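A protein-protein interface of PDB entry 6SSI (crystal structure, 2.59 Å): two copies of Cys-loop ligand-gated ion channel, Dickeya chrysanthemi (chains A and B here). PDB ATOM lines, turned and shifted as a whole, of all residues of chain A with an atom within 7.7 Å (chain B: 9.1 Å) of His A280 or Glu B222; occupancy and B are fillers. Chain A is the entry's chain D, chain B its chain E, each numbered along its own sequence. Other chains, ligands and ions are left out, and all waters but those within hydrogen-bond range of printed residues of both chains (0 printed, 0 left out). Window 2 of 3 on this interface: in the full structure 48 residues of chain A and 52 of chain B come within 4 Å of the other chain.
The side-chain hydroxyl (OG) of Ser A225 sits close to the side-chain carboxylate (OE1) of Glu B226, 3.2 Å away. A ring nitrogen (NE2) of His A280 is in hydrogen-bond range of the side-chain carboxylate (OE2) of Glu B222 (2.5 Å).
O of Phe B219 is in hydrogen-bond range of NE of Arg B297 (3.0 Å). The backbone carbonyl oxygen of Leu B221 sits at hydrogen-bond distance from the guanidinium group of Arg B227 (3.1 Å). The backbone carbonyl oxygen (O) of Glu B222 lies within hydrogen-bond range of the guanidinium group (NH1) of Arg B227, 3.2 Å away. The side-chain carboxylate of Glu B226 lies close to the side-chain hydroxyl of Ser B223, 3.1 Å away. The side-chain hydroxyl of Thr B230 is in hydrogen-bond range of the backbone carbonyl oxygen of Glu B226, at 2.7 Å.
Among the printed residues, pairs that only touch across the chains: Phe A224 with Trp B220, Leu A228 with Ser B217, Leu A228 with Leu B221, Ile A277 with Ser B217, Ile A277 with Trp B220, His A281 with Trp B220 and His A281 with Arg B297.
Of the printed residues of chain B, Ser A225 touches Glu B226 (3.1 Å). No residue of chain B comes within 4 Å of Ala A279. No residue of chain B comes within 4 Å of Gln A283. Of the printed residues of chain A, Leu B221 touches Leu A228 (3.7 Å). Glu B222 touches just one residue of chain A: His A280. The nearest residue of chain B that does not touch His A280 is Trp B220 (5.0 Å). The nearest printed residue of chain A that does not touch Trp B220 is Leu A228 (4.6 Å).
Of the 17 printed residues of chain B, 6 touch a printed residue of chain A. Of the 20 printed residues of chain A, 6 touch a printed residue of chain B.
Positions printed for both chains: 223, 224, 225, 227, 228, 280, 291 and 294. Of the 9 pairs that touch across the chains among the printed residues, none has its exchanged pair printed and touching as well.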
ATOM      1  N   SER A 223      23.818  33.281   5.886  1.00  0.00           N
ATOM      2  CA  SER A 223      23.164  33.017   4.609  1.00  0.00           C
ATOM      3  C   SER A 223      24.078  32.466   3.537  1.00  0.00           C
ATOM      4  O   SER A 223      25.285  32.730   3.538  1.00  0.00           O
ATOM      5  CB  SER A 223      22.452  34.269   4.105  1.00  0.00           C
ATOM      6  OG  SER A 223      23.377  35.258   3.692  1.00  0.00           O
ATOM      7  N   PHE A 224      23.479  31.715   2.602  1.00  0.00           N
ATOM      8  CA  PHE A 224      24.181  31.121   1.475  1.00  0.00           C
ATOM      9  C   PHE A 224      24.844  32.193   0.634  1.00  0.00           C
ATOM     10  O   PHE A 224      25.968  31.979   0.177  1.00  0.00           O
ATOM     11  CB  PHE A 224      23.237  30.272   0.626  1.00  0.00           C
ATOM     12  CG  PHE A 224      23.754  29.994  -0.762  1.00  0.00           C
ATOM     13  CD1 PHE A 224      24.679  28.986  -0.986  1.00  0.00           C
ATOM     14  CD2 PHE A 224      23.343  30.766  -1.841  1.00  0.00           C
ATOM     15  CE1 PHE A 224      25.140  28.717  -2.273  1.00  0.00           C
ATOM     16  CE2 PHE A 224      23.833  30.518  -3.121  1.00  0.00           C
ATOM     17  CZ  PHE A 224      24.706  29.479  -3.332  1.00  0.00           C
ATOM     18  N   SER A 225      24.154  33.340   0.436  1.00  0.00           N
ATOM     19  CA  SER A 225      24.670  34.468  -0.333  1.00  0.00           C
ATOM     20  C   SER A 225      25.966  34.985   0.283  1.00  0.00           C
ATOM     21  O   SER A 225      26.939  35.165  -0.447  1.00  0.00           O
ATOM     22  CB  SER A 225      23.631  35.579  -0.452  1.00  0.00           C
ATOM     23  OG  SER A 225      24.098  36.632  -1.282  1.00  0.00           O
ATOM     24  N   ARG A 227      28.051  33.300   2.504  1.00  0.00           N
ATOM     25  CA  ARG A 227      29.064  32.244   2.488  1.00  0.00           C
ATOM     26  C   ARG A 227      29.755  32.081   1.146  1.00  0.00           C
ATOM     27  O   ARG A 227      30.981  32.015   1.114  1.00  0.00           O
ATOM     28  CB  ARG A 227      28.493  30.906   2.956  1.00  0.00           C
ATOM     29  CG  ARG A 227      28.018  30.924   4.390  1.00  0.00           C
ATOM     30  CD  ARG A 227      27.596  29.552   4.882  1.00  0.00           C
ATOM     31  NE  ARG A 227      26.387  29.057   4.209  1.00  0.00           N
ATOM     32  CZ  ARG A 227      25.150  29.313   4.622  1.00  0.00           C
ATOM     33  NH1 ARG A 227      24.929  30.049   5.697  1.00  0.00           N
ATOM     34  NH2 ARG A 227      24.114  28.826   3.940  1.00  0.00           N
ATOM     35  N   LEU A 228      28.988  32.024   0.046  1.00  0.00           N
ATOM     36  CA  LEU A 228      29.546  31.854  -1.291  1.00  0.00           C
ATOM     37  C   LEU A 228      30.355  33.055  -1.744  1.00  0.00           C
ATOM     38  O   LEU A 228      31.477  32.878  -2.214  1.00  0.00           O
ATOM     39  CB  LEU A 228      28.461  31.506  -2.319  1.00  0.00           C
ATOM     40  CG  LEU A 228      28.952  31.094  -3.715  1.00  0.00           C
ATOM     41  CD1 LEU A 228      29.891  29.872  -3.662  1.00  0.00           C
ATOM     42  CD2 LEU A 228      27.795  30.814  -4.620  1.00  0.00           C
ATOM     43  N   LEU A 274      32.304  24.013  -2.462  1.00  0.00           N
ATOM     44  CA  LEU A 274      31.502  22.842  -2.800  1.00  0.00           C
ATOM     45  C   LEU A 274      30.484  22.539  -1.717  1.00  0.00           C
ATOM     46  O   LEU A 274      29.305  22.358  -2.026  1.00  0.00           O
ATOM     47  CB  LEU A 274      32.387  21.620  -3.106  1.00  0.00           C
ATOM     48  CG  LEU A 274      33.326  21.760  -4.321  1.00  0.00           C
ATOM     49  CD1 LEU A 274      34.264  20.590  -4.423  1.00  0.00           C
ATOM     50  CD2 LEU A 274      32.552  21.934  -5.621  1.00  0.00           C
ATOM     51  N   LEU A 275      30.925  22.563  -0.449  1.00  0.00           N
ATOM     52  CA  LEU A 275      30.077  22.308   0.711  1.00  0.00           C
ATOM     53  C   LEU A 275      28.964  23.337   0.804  1.00  0.00           C
ATOM     54  O   LEU A 275      27.799  22.964   0.963  1.00  0.00           O
ATOM     55  CB  LEU A 275      30.924  22.290   2.001  1.00  0.00           C
ATOM     56  CG  LEU A 275      31.468  20.931   2.496  1.00  0.00           C
ATOM     57  CD1 LEU A 275      30.362  20.036   3.022  1.00  0.00           C
ATOM     58  CD2 LEU A 275      32.320  20.215   1.444  1.00  0.00           C
ATOM     59  N   ILE A 276      29.317  24.621   0.629  1.00  0.00           N
ATOM     60  CA  ILE A 276      28.376  25.737   0.664  1.00  0.00           C
ATOM     61  C   ILE A 276      27.269  25.560  -0.382  1.00  0.00           C
ATOM     62  O   ILE A 276      26.096  25.815  -0.086  1.00  0.00           O
ATOM     63  CB  ILE A 276      29.125  27.103   0.553  1.00  0.00           C
ATOM     64  CG1 ILE A 276      29.939  27.376   1.837  1.00  0.00           C
ATOM     65  CG2 ILE A 276      28.161  28.271   0.266  1.00  0.00           C
ATOM     66  CD1 ILE A 276      31.035  28.417   1.710  1.00  0.00           C
ATOM     67  N   ILE A 277      27.640  25.123  -1.593  1.00  0.00           N
ATOM     68  CA  ILE A 277      26.669  24.945  -2.669  1.00  0.00           C
ATOM     69  C   ILE A 277      25.849  23.694  -2.453  1.00  0.00           C
ATOM     70  O   ILE A 277      24.627  23.730  -2.621  1.00  0.00           O
ATOM     71  CB  ILE A 277      27.310  25.028  -4.080  1.00  0.00           C
ATOM     72  CG1 ILE A 277      27.916  26.429  -4.300  1.00  0.00           C
ATOM     73  CG2 ILE A 277      26.267  24.732  -5.179  1.00  0.00           C
ATOM     74  CD1 ILE A 277      28.771  26.576  -5.487  1.00  0.00           C
ATOM     75  N   PHE A 278      26.507  22.599  -2.060  1.00  0.00           N
ATOM     76  CA  PHE A 278      25.822  21.339  -1.820  1.00  0.00           C
ATOM     77  C   PHE A 278      24.772  21.482  -0.724  1.00  0.00           C
ATOM     78  O   PHE A 278      23.704  20.888  -0.841  1.00  0.00           O
ATOM     79  CB  PHE A 278      26.816  20.209  -1.513  1.00  0.00           C
ATOM     80  CG  PHE A 278      26.176  18.857  -1.278  1.00  0.00           C
ATOM     81  CD1 PHE A 278      25.769  18.065  -2.347  1.00  0.00           C
ATOM     82  CD2 PHE A 278      25.958  18.386   0.013  1.00  0.00           C
ATOM     83  CE1 PHE A 278      25.165  16.820  -2.127  1.00  0.00           C
ATOM     84  CE2 PHE A 278      25.342  17.150   0.231  1.00  0.00           C
ATOM     85  CZ  PHE A 278      24.955  16.372  -0.839  1.00  0.00           C
ATOM     86  N   ALA A 279      25.064  22.279   0.317  1.00  0.00           N
ATOM     87  CA  ALA A 279      24.142  22.493   1.429  1.00  0.00           C
ATOM     88  C   ALA A 279      22.930  23.342   1.054  1.00  0.00           C
ATOM     89  O   ALA A 279      21.863  23.163   1.638  1.00  0.00           O
ATOM     90  CB  ALA A 279      24.874  23.119   2.597  1.00  0.00           C
ATOM     91  N   HIS A 280      23.077  24.253   0.096  1.00  0.00           N
ATOM     92  CA  HIS A 280      21.976  25.125  -0.289  1.00  0.00           C
ATOM     93  C   HIS A 280      20.944  24.475  -1.218  1.00  0.00           C
ATOM     94  O   HIS A 280      19.767  24.856  -1.188  1.00  0.00           O
ATOM     95  CB  HIS A 280      22.526  26.407  -0.887  1.00  0.00           C
ATOM     96  CG  HIS A 280      21.478  27.423  -1.210  1.00  0.00           C
ATOM     97  ND1 HIS A 280      20.709  28.015  -0.221  1.00  0.00           N
ATOM     98  CD2 HIS A 280      21.100  27.913  -2.411  1.00  0.00           C
ATOM     99  CE1 HIS A 280      19.897  28.841  -0.853  1.00  0.00           C
ATOM    100  NE2 HIS A 280      20.114  28.826  -2.166  1.00  0.00           N
ATOM    101  N   HIS A 281      21.378  23.507  -2.041  1.00  0.00           N
ATOM    102  CA  HIS A 281      20.506  22.810  -2.976  1.00  0.00           C
ATOM    103  C   HIS A 281      20.129  21.411  -2.477  1.00  0.00           C
ATOM    104  O   HIS A 281      19.396  20.695  -3.159  1.00  0.00           O
ATOM    105  CB  HIS A 281      21.110  22.815  -4.380  1.00  0.00           C
ATOM    106  CG  HIS A 281      20.969  24.140  -5.081  1.00  0.00           C
ATOM    107  ND1 HIS A 281      21.644  25.271  -4.643  1.00  0.00           N
ATOM    108  CD2 HIS A 281      20.246  24.465  -6.180  1.00  0.00           C
ATOM    109  CE1 HIS A 281      21.304  26.241  -5.478  1.00  0.00           C
ATOM    110  NE2 HIS A 281      20.468  25.805  -6.423  1.00  0.00           N
ATOM    111  N   ARG A 282      20.567  21.063  -1.251  1.00  0.00           N
ATOM    112  CA  ARG A 282      20.192  19.821  -0.584  1.00  0.00           C
ATOM    113  C   ARG A 282      19.000  20.143   0.300  1.00  0.00           C
ATOM    114  O   ARG A 282      18.293  19.217   0.689  1.00  0.00           O
ATOM    115  CB  ARG A 282      21.333  19.216   0.247  1.00  0.00           C
ATOM    116  N   GLN A 283      18.760  21.460   0.597  1.00  0.00           N
ATOM    117  CA  GLN A 283      17.636  21.979   1.397  1.00  0.00           C
ATOM    118  C   GLN A 283      16.317  21.802   0.622  1.00  0.00           C
ATOM    119  O   GLN A 283      15.747  22.784   0.125  1.00  0.00           O
ATOM    120  CB  GLN A 283      17.855  23.464   1.759  1.00  0.00           C
ATOM    121  N   ALA A 284      15.873  20.530   0.472  1.00  0.00           N
ATOM    122  CA  ALA A 284      14.657  20.162  -0.253  1.00  0.00           C
ATOM    123  C   ALA A 284      13.455  20.582   0.554  1.00  0.00           C
ATOM    124  O   ALA A 284      12.534  21.174  -0.012  1.00  0.00           O
ATOM    125  CB  ALA A 284      14.623  18.667  -0.534  1.00  0.00           C
ATOM    126  N   ASP A 290      19.390  22.866   4.317  1.00  0.00           N
ATOM    127  CA  ASP A 290      20.255  21.896   4.972  1.00  0.00           C
ATOM    128  C   ASP A 290      21.098  22.591   6.037  1.00  0.00           C
ATOM    129  O   ASP A 290      22.334  22.639   5.951  1.00  0.00           O
ATOM    130  CB  ASP A 290      21.118  21.145   3.947  1.00  0.00           C
ATOM    131  N   LEU A 291      20.404  23.135   7.057  1.00  0.00           N
ATOM    132  CA  LEU A 291      21.017  23.845   8.181  1.00  0.00           C
ATOM    133  C   LEU A 291      21.960  22.951   8.992  1.00  0.00           C
ATOM    134  O   LEU A 291      22.887  23.468   9.622  1.00  0.00           O
ATOM    135  CB  LEU A 291      19.947  24.470   9.091  1.00  0.00           C
ATOM    136  N   ILE A 293      24.130  20.374   7.825  1.00  0.00           N
ATOM    137  CA  ILE A 293      25.431  20.291   7.160  1.00  0.00           C
ATOM    138  C   ILE A 293      26.193  21.594   7.243  1.00  0.00           C
ATOM    139  O   ILE A 293      27.409  21.555   7.434  1.00  0.00           O
ATOM    140  CB  ILE A 293      25.320  19.786   5.707  1.00  0.00           C
ATOM    141  N   GLN A 294      25.478  22.745   7.153  1.00  0.00           N
ATOM    142  CA  GLN A 294      26.051  24.094   7.247  1.00  0.00           C
ATOM    143  C   GLN A 294      26.874  24.258   8.530  1.00  0.00           C
ATOM    144  O   GLN A 294      27.848  25.014   8.537  1.00  0.00           O
ATOM    145  CB  GLN A 294      24.960  25.178   7.144  1.00  0.00           C
ATOM    146  N   SER B 217      30.704  28.859 -10.268  1.00  0.00           N
ATOM    147  CA  SER B 217      29.727  28.857  -9.180  1.00  0.00           C
ATOM    148  C   SER B 217      28.869  30.131  -9.130  1.00  0.00           C
ATOM    149  O   SER B 217      27.939  30.204  -8.323  1.00  0.00           O
ATOM    150  CB  SER B 217      30.422  28.619  -7.848  1.00  0.00           C
ATOM    151  OG  SER B 217      31.220  29.729  -7.479  1.00  0.00           O
ATOM    152  N   VAL B 218      29.169  31.121 -10.003  1.00  0.00           N
ATOM    153  CA  VAL B 218      28.427  32.379 -10.127  1.00  0.00           C
ATOM    154  C   VAL B 218      26.961  32.090 -10.467  1.00  0.00           C
ATOM    155  O   VAL B 218      26.069  32.775  -9.966  1.00  0.00           O
ATOM    156  CB  VAL B 218      29.101  33.376 -11.125  1.00  0.00           C
ATOM    157  CG1 VAL B 218      29.111  32.852 -12.565  1.00  0.00           C
ATOM    158  CG2 VAL B 218      28.462  34.753 -11.053  1.00  0.00           C
ATOM    159  N   PHE B 219      26.728  31.044 -11.283  1.00  0.00           N
ATOM    160  CA  PHE B 219      25.402  30.628 -11.721  1.00  0.00           C
ATOM    161  C   PHE B 219      24.559  30.033 -10.607  1.00  0.00           C
ATOM    162  O   PHE B 219      23.367  29.816 -10.818  1.00  0.00           O
ATOM    163  CB  PHE B 219      25.490  29.662 -12.908  1.00  0.00           C
ATOM    164  CG  PHE B 219      26.253  30.207 -14.080  1.00  0.00           C
ATOM    165  CD1 PHE B 219      25.785  31.310 -14.782  1.00  0.00           C
ATOM    166  CD2 PHE B 219      27.436  29.616 -14.489  1.00  0.00           C
ATOM    167  CE1 PHE B 219      26.495  31.817 -15.865  1.00  0.00           C
ATOM    168  CE2 PHE B 219      28.159  30.138 -15.556  1.00  0.00           C
ATOM    169  CZ  PHE B 219      27.675  31.225 -16.248  1.00  0.00           C
ATOM    170  N   TRP B 220      25.150  29.817  -9.417  1.00  0.00           N
ATOM    171  CA  TRP B 220      24.452  29.271  -8.255  1.00  0.00           C
ATOM    172  C   TRP B 220      23.953  30.346  -7.307  1.00  0.00           C
ATOM    173  O   TRP B 220      23.187  30.043  -6.385  1.00  0.00           O
ATOM    174  CB  TRP B 220      25.297  28.228  -7.538  1.00  0.00           C
ATOM    175  CG  TRP B 220      25.586  27.036  -8.395  1.00  0.00           C
ATOM    176  CD1 TRP B 220      26.588  26.913  -9.311  1.00  0.00           C
ATOM    177  CD2 TRP B 220      24.846  25.809  -8.443  1.00  0.00           C
ATOM    178  NE1 TRP B 220      26.537  25.675  -9.905  1.00  0.00           N
ATOM    179  CE2 TRP B 220      25.490  24.968  -9.376  1.00  0.00           C
ATOM    180  CE3 TRP B 220      23.706  25.328  -7.774  1.00  0.00           C
ATOM    181  CZ2 TRP B 220      25.028  23.678  -9.666  1.00  0.00           C
ATOM    182  CZ3 TRP B 220      23.261  24.045  -8.051  1.00  0.00           C
ATOM    183  CH2 TRP B 220      23.908  23.241  -8.998  1.00  0.00           C
ATOM    184  N   LEU B 221      24.331  31.611  -7.567  1.00  0.00           N
ATOM    185  CA  LEU B 221      23.845  32.747  -6.790  1.00  0.00           C
ATOM    186  C   LEU B 221      22.410  32.989  -7.224  1.00  0.00           C
ATOM    187  O   LEU B 221      22.055  32.713  -8.373  1.00  0.00           O
ATOM    188  CB  LEU B 221      24.723  33.990  -6.948  1.00  0.00           C
ATOM    189  CG  LEU B 221      26.114  33.899  -6.336  1.00  0.00           C
ATOM    190  CD1 LEU B 221      26.995  34.944  -6.918  1.00  0.00           C
ATOM    191  CD2 LEU B 221      26.072  34.027  -4.812  1.00  0.00           C
ATOM    192  N   GLU B 222      21.574  33.422  -6.283  1.00  0.00           N
ATOM    193  CA  GLU B 222      20.130  33.547  -6.455  1.00  0.00           C
ATOM    194  C   GLU B 222      19.625  34.756  -7.215  1.00  0.00           C
ATOM    195  O   GLU B 222      18.619  34.653  -7.923  1.00  0.00           O
ATOM    196  CB  GLU B 222      19.449  33.491  -5.086  1.00  0.00           C
ATOM    197  CG  GLU B 222      19.815  32.238  -4.306  1.00  0.00           C
ATOM    198  CD  GLU B 222      19.281  30.923  -4.848  1.00  0.00           C
ATOM    199  OE1 GLU B 222      19.239  30.724  -6.085  1.00  0.00           O
ATOM    200  OE2 GLU B 222      18.889  30.082  -4.014  1.00  0.00           O
ATOM    201  N   SER B 223      20.260  35.901  -7.028  1.00  0.00           N
ATOM    202  CA  SER B 223      19.795  37.117  -7.673  1.00  0.00           C
ATOM    203  C   SER B 223      20.747  37.578  -8.744  1.00  0.00           C
ATOM    204  O   SER B 223      21.941  37.286  -8.677  1.00  0.00           O
ATOM    205  CB  SER B 223      19.609  38.224  -6.639  1.00  0.00           C
ATOM    206  OG  SER B 223      20.851  38.618  -6.084  1.00  0.00           O
ATOM    207  N   PHE B 224      20.217  38.350  -9.707  1.00  0.00           N
ATOM    208  CA  PHE B 224      20.967  38.964 -10.796  1.00  0.00           C
ATOM    209  C   PHE B 224      22.023  39.916 -10.256  1.00  0.00           C
ATOM    210  O   PHE B 224      23.128  39.951 -10.794  1.00  0.00           O
ATOM    211  CB  PHE B 224      20.026  39.701 -11.753  1.00  0.00           C
ATOM    212  CG  PHE B 224      20.694  40.723 -12.641  1.00  0.00           C
ATOM    213  CD1 PHE B 224      21.424  40.328 -13.754  1.00  0.00           C
ATOM    214  CD2 PHE B 224      20.613  42.079 -12.351  1.00  0.00           C
ATOM    215  CE1 PHE B 224      22.035  41.273 -14.580  1.00  0.00           C
ATOM    216  CE2 PHE B 224      21.223  43.025 -13.178  1.00  0.00           C
ATOM    217  CZ  PHE B 224      21.921  42.616 -14.293  1.00  0.00           C
ATOM    218  N   SER B 225      21.680  40.690  -9.204  1.00  0.00           N
ATOM    219  CA  SER B 225      22.588  41.627  -8.557  1.00  0.00           C
ATOM    220  C   SER B 225      23.811  40.901  -7.993  1.00  0.00           C
ATOM    221  O   SER B 225      24.928  41.351  -8.234  1.00  0.00           O
ATOM    222  CB  SER B 225      21.877  42.414  -7.464  1.00  0.00           C
ATOM    223  OG  SER B 225      22.778  43.346  -6.894  1.00  0.00           O
ATOM    224  N   GLU B 226      23.610  39.744  -7.328  1.00  0.00           N
ATOM    225  CA  GLU B 226      24.693  38.945  -6.756  1.00  0.00           C
ATOM    226  C   GLU B 226      25.599  38.364  -7.826  1.00  0.00           C
ATOM    227  O   GLU B 226      26.811  38.426  -7.665  1.00  0.00           O
ATOM    228  CB  GLU B 226      24.155  37.814  -5.875  1.00  0.00           C
ATOM    229  CG  GLU B 226      23.519  38.261  -4.570  1.00  0.00           C
ATOM    230  CD  GLU B 226      22.617  37.208  -3.955  1.00  0.00           C
ATOM    231  OE1 GLU B 226      22.865  36.002  -4.183  1.00  0.00           O
ATOM    232  OE2 GLU B 226      21.657  37.585  -3.246  1.00  0.00           O
ATOM    233  N   ARG B 227      25.027  37.821  -8.913  1.00  0.00           N
ATOM    234  CA  ARG B 227      25.786  37.214 -10.008  1.00  0.00           C
ATOM    235  C   ARG B 227      26.681  38.196 -10.738  1.00  0.00           C
ATOM    236  O   ARG B 227      27.851  37.894 -10.944  1.00  0.00           O
ATOM    237  CB  ARG B 227      24.866  36.492 -10.988  1.00  0.00           C
ATOM    238  CG  ARG B 227      24.084  35.407 -10.304  1.00  0.00           C
ATOM    239  CD  ARG B 227      23.313  34.577 -11.275  1.00  0.00           C
ATOM    240  NE  ARG B 227      22.221  35.322 -11.904  1.00  0.00           N
ATOM    241  CZ  ARG B 227      20.962  35.298 -11.479  1.00  0.00           C
ATOM    242  NH1 ARG B 227      20.616  34.606 -10.409  1.00  0.00           N
ATOM    243  NH2 ARG B 227      20.037  36.010 -12.121  1.00  0.00           N
ATOM    244  N   LEU B 228      26.151  39.368 -11.108  1.00  0.00           N
ATOM    245  CA  LEU B 228      26.918  40.378 -11.822  1.00  0.00           C
ATOM    246  C   LEU B 228      28.027  40.996 -10.981  1.00  0.00           C
ATOM    247  O   LEU B 228      29.129  41.177 -11.497  1.00  0.00           O
ATOM    248  CB  LEU B 228      26.007  41.457 -12.420  1.00  0.00           C
ATOM    249  CG  LEU B 228      26.666  42.469 -13.374  1.00  0.00           C
ATOM    250  CD1 LEU B 228      27.395  41.768 -14.533  1.00  0.00           C
ATOM    251  CD2 LEU B 228      25.646  43.443 -13.917  1.00  0.00           C
ATOM    252  N   THR B 230      29.505  39.600  -8.269  1.00  0.00           N
ATOM    253  CA  THR B 230      30.475  38.553  -7.949  1.00  0.00           C
ATOM    254  C   THR B 230      31.407  38.329  -9.133  1.00  0.00           C
ATOM    255  O   THR B 230      32.565  37.953  -8.927  1.00  0.00           O
ATOM    256  CB  THR B 230      29.747  37.281  -7.518  1.00  0.00           C
ATOM    257  OG1 THR B 230      29.037  37.555  -6.312  1.00  0.00           O
ATOM    258  CG2 THR B 230      30.669  36.122  -7.282  1.00  0.00           C
ATOM    259  N   HIS B 280      18.726  38.122 -17.724  1.00  0.00           N
ATOM    260  CA  HIS B 280      17.920  39.127 -17.044  1.00  0.00           C
ATOM    261  C   HIS B 280      17.063  40.037 -17.943  1.00  0.00           C
ATOM    262  O   HIS B 280      16.015  40.515 -17.502  1.00  0.00           O
ATOM    263  CB  HIS B 280      18.827  39.973 -16.180  1.00  0.00           C
ATOM    264  CG  HIS B 280      18.095  40.744 -15.133  1.00  0.00           C
ATOM    265  ND1 HIS B 280      17.540  40.116 -14.028  1.00  0.00           N
ATOM    266  CD2 HIS B 280      17.869  42.075 -15.044  1.00  0.00           C
ATOM    267  CE1 HIS B 280      17.014  41.084 -13.297  1.00  0.00           C
ATOM    268  NE2 HIS B 280      17.184  42.279 -13.872  1.00  0.00           N
ATOM    269  N   LEU B 291      15.219  32.132 -15.593  1.00  0.00           N
ATOM    270  CA  LEU B 291      16.017  31.342 -14.660  1.00  0.00           C
ATOM    271  C   LEU B 291      16.321  29.939 -15.193  1.00  0.00           C
ATOM    272  O   LEU B 291      17.051  29.186 -14.542  1.00  0.00           O
ATOM    273  CB  LEU B 291      15.336  31.283 -13.289  1.00  0.00           C
ATOM    274  CG  LEU B 291      15.109  32.628 -12.611  1.00  0.00           C
ATOM    275  CD1 LEU B 291      13.752  32.675 -11.960  1.00  0.00           C
ATOM    276  CD2 LEU B 291      16.239  32.962 -11.641  1.00  0.00           C
ATOM    277  N   GLN B 294      19.759  30.026 -16.529  1.00  0.00           N
ATOM    278  CA  GLN B 294      20.567  30.073 -15.316  1.00  0.00           C
ATOM    279  C   GLN B 294      20.985  28.677 -14.900  1.00  0.00           C
ATOM    280  O   GLN B 294      21.986  28.529 -14.199  1.00  0.00           O
ATOM    281  CB  GLN B 294      19.812  30.775 -14.186  1.00  0.00           C
ATOM    282  CG  GLN B 294      20.698  31.640 -13.332  1.00  0.00           C
ATOM    283  CD  GLN B 294      21.342  32.767 -14.108  1.00  0.00           C
ATOM    284  OE1 GLN B 294      22.396  33.241 -13.731  1.00  0.00           O
ATOM    285  NE2 GLN B 294      20.760  33.227 -15.213  1.00  0.00           N
ATOM    286  N   ARG B 297      24.536  25.903 -15.326  1.00  0.00           N
ATOM    287  CA  ARG B 297      25.512  25.550 -14.293  1.00  0.00           C
ATOM    288  C   ARG B 297      26.280  24.314 -14.754  1.00  0.00           C
ATOM    289  O   ARG B 297      27.407  24.108 -14.326  1.00  0.00           O
ATOM    290  CB  ARG B 297      24.818  25.243 -12.962  1.00  0.00           C
ATOM    291  CG  ARG B 297      24.069  26.413 -12.359  1.00  0.00           C
ATOM    292  CD  ARG B 297      22.847  25.963 -11.600  1.00  0.00           C
ATOM    293  NE  ARG B 297      22.180  27.107 -10.978  1.00  0.00           N
ATOM    294  CZ  ARG B 297      21.091  27.022 -10.223  1.00  0.00           C
ATOM    295  NH1 ARG B 297      20.533  25.847  -9.970  1.00  0.00           N
ATOM    296  NH2 ARG B 297      20.552  28.122  -9.706  1.00  0.00           N
